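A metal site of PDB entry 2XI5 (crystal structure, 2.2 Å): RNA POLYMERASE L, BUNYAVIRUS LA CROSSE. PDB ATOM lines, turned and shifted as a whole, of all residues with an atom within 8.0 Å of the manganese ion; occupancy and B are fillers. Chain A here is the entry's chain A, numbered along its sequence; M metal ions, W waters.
N of Asp 80 sits at hydrogen-bond distance from O of Ile 92 (3.3 Å).
The side-chain hydroxyl (OH) of Tyr 94 lies within hydrogen-bond range of the side-chain amide nitrogen (ND2) of Asn 81 (2.9 Å).
OD2 of Asp 93 lies within salt-bridge range of NZ of Lys 95 (2.6 Å).
The backbone carbonyl oxygen of Asp 93 sits at hydrogen-bond distance from the backbone NH of Ile 130 (2.8 Å).
The side-chain carboxylate of Asp 36 sits at hydrogen-bond distance from a ring nitrogen (ND1) of His 35 (2.9 Å).
The manganese ion is bound by OD2 of Asp 80, O of Tyr 94, water W1, OD1 of Asp 93 and NE2 of His 35.
Slightly farther from the manganese ion lies water W2 (2.7 Å).
Within 4 Å of the manganese ion: His 35, Asp 80, Asp 93 and Tyr 94.
The nearest printed residue that does not touch the manganese ion is Lys 95 (4.1 Å).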
ATOM      1  N   MET A  32      -4.552 -20.813   9.160  1.00  0.00           N
ATOM      2  CA  MET A  32      -4.572 -22.270   9.350  1.00  0.00           C
ATOM      3  C   MET A  32      -3.494 -22.685  10.369  1.00  0.00           C
ATOM      4  O   MET A  32      -3.755 -23.497  11.228  1.00  0.00           O
ATOM      5  CB  MET A  32      -4.373 -23.059   8.050  1.00  0.00           C
ATOM      6  CG  MET A  32      -4.546 -24.589   8.212  1.00  0.00           C
ATOM      7  SD  MET A  32      -6.141 -25.159   8.871  1.00  0.00           S
ATOM      8  CE  MET A  32      -5.867 -26.937   8.971  1.00  0.00           C
ATOM      9  N   HIS A  35      -4.685 -21.828  13.993  1.00  0.00           N
ATOM     10  CA  HIS A  35      -5.669 -22.792  14.432  1.00  0.00           C
ATOM     11  C   HIS A  35      -4.994 -24.102  14.828  1.00  0.00           C
ATOM     12  O   HIS A  35      -5.351 -24.683  15.826  1.00  0.00           O
ATOM     13  CB  HIS A  35      -6.660 -23.006  13.291  1.00  0.00           C
ATOM     14  CG  HIS A  35      -7.531 -24.233  13.398  1.00  0.00           C
ATOM     15  ND1 HIS A  35      -7.102 -25.475  12.998  1.00  0.00           N
ATOM     16  CD2 HIS A  35      -8.854 -24.355  13.670  1.00  0.00           C
ATOM     17  CE1 HIS A  35      -8.099 -26.335  13.118  1.00  0.00           C
ATOM     18  NE2 HIS A  35      -9.177 -25.685  13.531  1.00  0.00           N
ATOM     19  N   ASP A  36      -4.048 -24.569  14.017  1.00  0.00           N
ATOM     20  CA  ASP A  36      -3.325 -25.817  14.289  1.00  0.00           C
ATOM     21  C   ASP A  36      -2.438 -25.726  15.541  1.00  0.00           C
ATOM     22  O   ASP A  36      -2.350 -26.673  16.315  1.00  0.00           O
ATOM     23  CB  ASP A  36      -2.527 -26.273  13.046  1.00  0.00           C
ATOM     24  CG  ASP A  36      -3.436 -26.707  11.905  1.00  0.00           C
ATOM     25  OD1 ASP A  36      -4.680 -26.751  12.104  1.00  0.00           O
ATOM     26  OD2 ASP A  36      -2.912 -27.004  10.810  1.00  0.00           O
ATOM     27  N   PHE A  38      -3.075 -23.715  18.101  1.00  0.00           N
ATOM     28  CA  PHE A  38      -3.998 -23.849  19.230  1.00  0.00           C
ATOM     29  C   PHE A  38      -4.396 -25.297  19.487  1.00  0.00           C
ATOM     30  O   PHE A  38      -4.412 -25.739  20.610  1.00  0.00           O
ATOM     31  CB  PHE A  38      -5.242 -23.026  18.995  1.00  0.00           C
ATOM     32  CG  PHE A  38      -6.317 -23.234  19.980  1.00  0.00           C
ATOM     33  CD1 PHE A  38      -6.086 -23.123  21.323  1.00  0.00           C
ATOM     34  CD2 PHE A  38      -7.565 -23.541  19.548  1.00  0.00           C
ATOM     35  CE1 PHE A  38      -7.100 -23.293  22.224  1.00  0.00           C
ATOM     36  CE2 PHE A  38      -8.620 -23.711  20.459  1.00  0.00           C
ATOM     37  CZ  PHE A  38      -8.381 -23.582  21.790  1.00  0.00           C
ATOM     38  N   THR A  78     -14.969 -34.797   8.752  1.00  0.00           N
ATOM     39  CA  THR A  78     -13.631 -34.989   9.333  1.00  0.00           C
ATOM     40  C   THR A  78     -13.414 -33.938  10.406  1.00  0.00           C
ATOM     41  O   THR A  78     -12.999 -32.830  10.121  1.00  0.00           O
ATOM     42  CB  THR A  78     -12.525 -34.917   8.302  1.00  0.00           C
ATOM     43  OG1 THR A  78     -12.762 -35.928   7.324  1.00  0.00           O
ATOM     44  CG2 THR A  78     -11.127 -35.148   8.951  1.00  0.00           C
ATOM     45  N   PRO A  79     -13.750 -34.285  11.655  1.00  0.00           N
ATOM     46  CA  PRO A  79     -13.610 -33.348  12.751  1.00  0.00           C
ATOM     47  C   PRO A  79     -12.166 -33.236  13.179  1.00  0.00           C
ATOM     48  O   PRO A  79     -11.369 -34.159  12.938  1.00  0.00           O
ATOM     49  CB  PRO A  79     -14.431 -33.956  13.882  1.00  0.00           C
ATOM     50  CG  PRO A  79     -14.604 -35.390  13.513  1.00  0.00           C
ATOM     51  CD  PRO A  79     -14.334 -35.561  12.055  1.00  0.00           C
ATOM     52  N   ASP A  80     -11.811 -32.125  13.798  1.00  0.00           N
ATOM     53  CA  ASP A  80     -10.433 -31.946  14.285  1.00  0.00           C
ATOM     54  C   ASP A  80     -10.020 -33.093  15.245  1.00  0.00           C
ATOM     55  O   ASP A  80      -8.896 -33.543  15.199  1.00  0.00           O
ATOM     56  CB  ASP A  80     -10.277 -30.638  15.009  1.00  0.00           C
ATOM     57  CG  ASP A  80     -10.429 -29.411  14.098  1.00  0.00           C
ATOM     58  OD1 ASP A  80     -10.142 -29.479  12.908  1.00  0.00           O
ATOM     59  OD2 ASP A  80     -10.821 -28.349  14.632  1.00  0.00           O
ATOM     60  N   ASN A  81     -10.926 -33.564  16.103  1.00  0.00           N
ATOM     61  CA  ASN A  81     -10.520 -34.559  17.081  1.00  0.00           C
ATOM     62  C   ASN A  81     -11.746 -35.209  17.662  1.00  0.00           C
ATOM     63  O   ASN A  81     -12.875 -34.795  17.366  1.00  0.00           O
ATOM     64  CB  ASN A  81      -9.675 -33.878  18.195  1.00  0.00           C
ATOM     65  CG  ASN A  81      -8.563 -34.817  18.781  1.00  0.00           C
ATOM     66  OD1 ASN A  81      -8.756 -36.030  18.852  1.00  0.00           O
ATOM     67  ND2 ASN A  81      -7.430 -34.226  19.211  1.00  0.00           N
ATOM     68  N   ILE A  92     -14.911 -33.220  18.450  1.00  0.00           N
ATOM     69  CA  ILE A  92     -14.274 -31.992  18.871  1.00  0.00           C
ATOM     70  C   ILE A  92     -13.843 -31.152  17.694  1.00  0.00           C
ATOM     71  O   ILE A  92     -13.150 -31.640  16.791  1.00  0.00           O
ATOM     72  CB  ILE A  92     -13.028 -32.315  19.755  1.00  0.00           C
ATOM     73  CG1 ILE A  92     -13.425 -33.022  21.044  1.00  0.00           C
ATOM     74  CG2 ILE A  92     -12.296 -31.087  20.140  1.00  0.00           C
ATOM     75  CD1 ILE A  92     -12.256 -33.580  21.817  1.00  0.00           C
ATOM     76  N   ASP A  93     -14.174 -29.881  17.746  1.00  0.00           N
ATOM     77  CA  ASP A  93     -13.650 -28.886  16.773  1.00  0.00           C
ATOM     78  C   ASP A  93     -12.919 -27.734  17.469  1.00  0.00           C
ATOM     79  O   ASP A  93     -13.393 -27.180  18.437  1.00  0.00           O
ATOM     80  CB  ASP A  93     -14.785 -28.345  15.887  1.00  0.00           C
ATOM     81  CG  ASP A  93     -14.326 -27.208  14.950  1.00  0.00           C
ATOM     82  OD1 ASP A  93     -13.537 -27.480  14.017  1.00  0.00           O
ATOM     83  OD2 ASP A  93     -14.797 -26.052  15.160  1.00  0.00           O
ATOM     84  N   TYR A  94     -11.757 -27.359  16.949  1.00  0.00           N
ATOM     85  CA  TYR A  94     -11.041 -26.207  17.445  1.00  0.00           C
ATOM     86  C   TYR A  94     -11.510 -24.956  16.679  1.00  0.00           C
ATOM     87  O   TYR A  94     -11.758 -25.050  15.491  1.00  0.00           O
ATOM     88  CB  TYR A  94      -9.521 -26.389  17.202  1.00  0.00           C
ATOM     89  CG  TYR A  94      -8.918 -27.775  17.505  1.00  0.00           C
ATOM     90  CD1 TYR A  94      -9.214 -28.444  18.642  1.00  0.00           C
ATOM     91  CD2 TYR A  94      -7.976 -28.342  16.671  1.00  0.00           C
ATOM     92  CE1 TYR A  94      -8.651 -29.674  18.923  1.00  0.00           C
ATOM     93  CE2 TYR A  94      -7.419 -29.546  16.920  1.00  0.00           C
ATOM     94  CZ  TYR A  94      -7.744 -30.220  18.059  1.00  0.00           C
ATOM     95  OH  TYR A  94      -7.173 -31.465  18.322  1.00  0.00           O
ATOM     96  N   LYS A  95     -11.590 -23.804  17.338  1.00  0.00           N
ATOM     97  CA  LYS A  95     -11.784 -22.515  16.693  1.00  0.00           C
ATOM     98  C   LYS A  95     -10.903 -21.470  17.345  1.00  0.00           C
ATOM     99  O   LYS A  95     -10.735 -21.480  18.559  1.00  0.00           O
ATOM    100  CB  LYS A  95     -13.225 -22.038  16.812  1.00  0.00           C
ATOM    101  CG  LYS A  95     -14.198 -22.798  15.990  1.00  0.00           C
ATOM    102  CD  LYS A  95     -14.041 -22.504  14.488  1.00  0.00           C
ATOM    103  CE  LYS A  95     -15.172 -23.065  13.632  1.00  0.00           C
ATOM    104  NZ  LYS A  95     -15.012 -24.480  13.117  1.00  0.00           N
ATOM    105  N   VAL A  96     -10.357 -20.578  16.541  1.00  0.00           N
ATOM    106  CA  VAL A  96      -9.681 -19.381  17.047  1.00  0.00           C
ATOM    107  C   VAL A  96     -10.455 -18.216  16.435  1.00  0.00           C
ATOM    108  O   VAL A  96     -10.390 -18.008  15.235  1.00  0.00           O
ATOM    109  CB  VAL A  96      -8.207 -19.302  16.641  1.00  0.00           C
ATOM    110  CG1 VAL A  96      -7.509 -18.025  17.202  1.00  0.00           C
ATOM    111  CG2 VAL A  96      -7.445 -20.580  17.100  1.00  0.00           C
ATOM    112  N   SER A 102     -18.523 -18.827  13.289  1.00  0.00           N
ATOM    113  CA  SER A 102     -18.011 -20.044  12.642  1.00  0.00           C
ATOM    114  C   SER A 102     -18.346 -21.251  13.508  1.00  0.00           C
ATOM    115  O   SER A 102     -18.601 -22.308  12.991  1.00  0.00           O
ATOM    116  CB  SER A 102     -16.478 -19.957  12.406  1.00  0.00           C
ATOM    117  OG  SER A 102     -15.769 -19.770  13.630  1.00  0.00           O
ATOM    118  N   THR A 106     -20.363 -24.868  12.315  1.00  0.00           N
ATOM    119  CA  THR A 106     -19.800 -26.192  12.494  1.00  0.00           C
ATOM    120  C   THR A 106     -20.673 -27.019  13.443  1.00  0.00           C
ATOM    121  O   THR A 106     -20.993 -28.153  13.141  1.00  0.00           O
ATOM    122  CB  THR A 106     -18.348 -26.108  13.025  1.00  0.00           C
ATOM    123  OG1 THR A 106     -17.555 -25.311  12.135  1.00  0.00           O
ATOM    124  CG2 THR A 106     -17.723 -27.443  13.133  1.00  0.00           C
ATOM    125  N   TYR A 110     -22.342 -30.573  12.260  1.00  0.00           N
ATOM    126  CA  TYR A 110     -21.923 -31.789  12.950  1.00  0.00           C
ATOM    127  C   TYR A 110     -23.059 -32.401  13.803  1.00  0.00           C
ATOM    128  O   TYR A 110     -23.224 -33.623  13.878  1.00  0.00           O
ATOM    129  CB  TYR A 110     -20.713 -31.473  13.861  1.00  0.00           C
ATOM    130  CG  TYR A 110     -19.375 -31.286  13.196  1.00  0.00           C
ATOM    131  CD1 TYR A 110     -19.239 -31.212  11.825  1.00  0.00           C
ATOM    132  CD2 TYR A 110     -18.232 -31.193  13.968  1.00  0.00           C
ATOM    133  CE1 TYR A 110     -17.979 -31.027  11.252  1.00  0.00           C
ATOM    134  CE2 TYR A 110     -17.013 -31.021  13.411  1.00  0.00           C
ATOM    135  CZ  TYR A 110     -16.875 -30.937  12.049  1.00  0.00           C
ATOM    136  OH  TYR A 110     -15.639 -30.768  11.490  1.00  0.00           O
ATOM    137  N   ILE A 129     -17.393 -27.681  20.570  1.00  0.00           N
ATOM    138  CA  ILE A 129     -16.608 -26.668  19.895  1.00  0.00           C
ATOM    139  C   ILE A 129     -15.770 -26.005  20.963  1.00  0.00           C
ATOM    140  O   ILE A 129     -16.310 -25.431  21.889  1.00  0.00           O
ATOM    141  CB  ILE A 129     -17.477 -25.614  19.193  1.00  0.00           C
ATOM    142  CG1 ILE A 129     -18.578 -26.263  18.335  1.00  0.00           C
ATOM    143  CG2 ILE A 129     -16.674 -24.710  18.363  1.00  0.00           C
ATOM    144  CD1 ILE A 129     -18.139 -27.088  17.154  1.00  0.00           C
ATOM    145  N   ILE A 130     -14.451 -26.123  20.854  1.00  0.00           N
ATOM    146  CA  ILE A 130     -13.537 -25.435  21.770  1.00  0.00           C
ATOM    147  C   ILE A 130     -12.943 -24.191  21.098  1.00  0.00           C
ATOM    148  O   ILE A 130     -12.149 -24.288  20.164  1.00  0.00           O
ATOM    149  CB  ILE A 130     -12.449 -26.374  22.236  1.00  0.00           C
ATOM    150  CG1 ILE A 130     -13.082 -27.618  22.861  1.00  0.00           C
ATOM    151  CG2 ILE A 130     -11.507 -25.680  23.251  1.00  0.00           C
ATOM    152  CD1 ILE A 130     -12.078 -28.717  23.286  1.00  0.00           C
HETATM  153 MN    MN M   1     -11.474 -26.415  13.638  1.00  0.00          MN
HETATM  154  O   HOH W   1     -11.318 -27.533  11.591  1.00  0.00           O
HETATM  155  O   HOH W   2     -12.162 -24.408  11.912  1.00  0.00           O
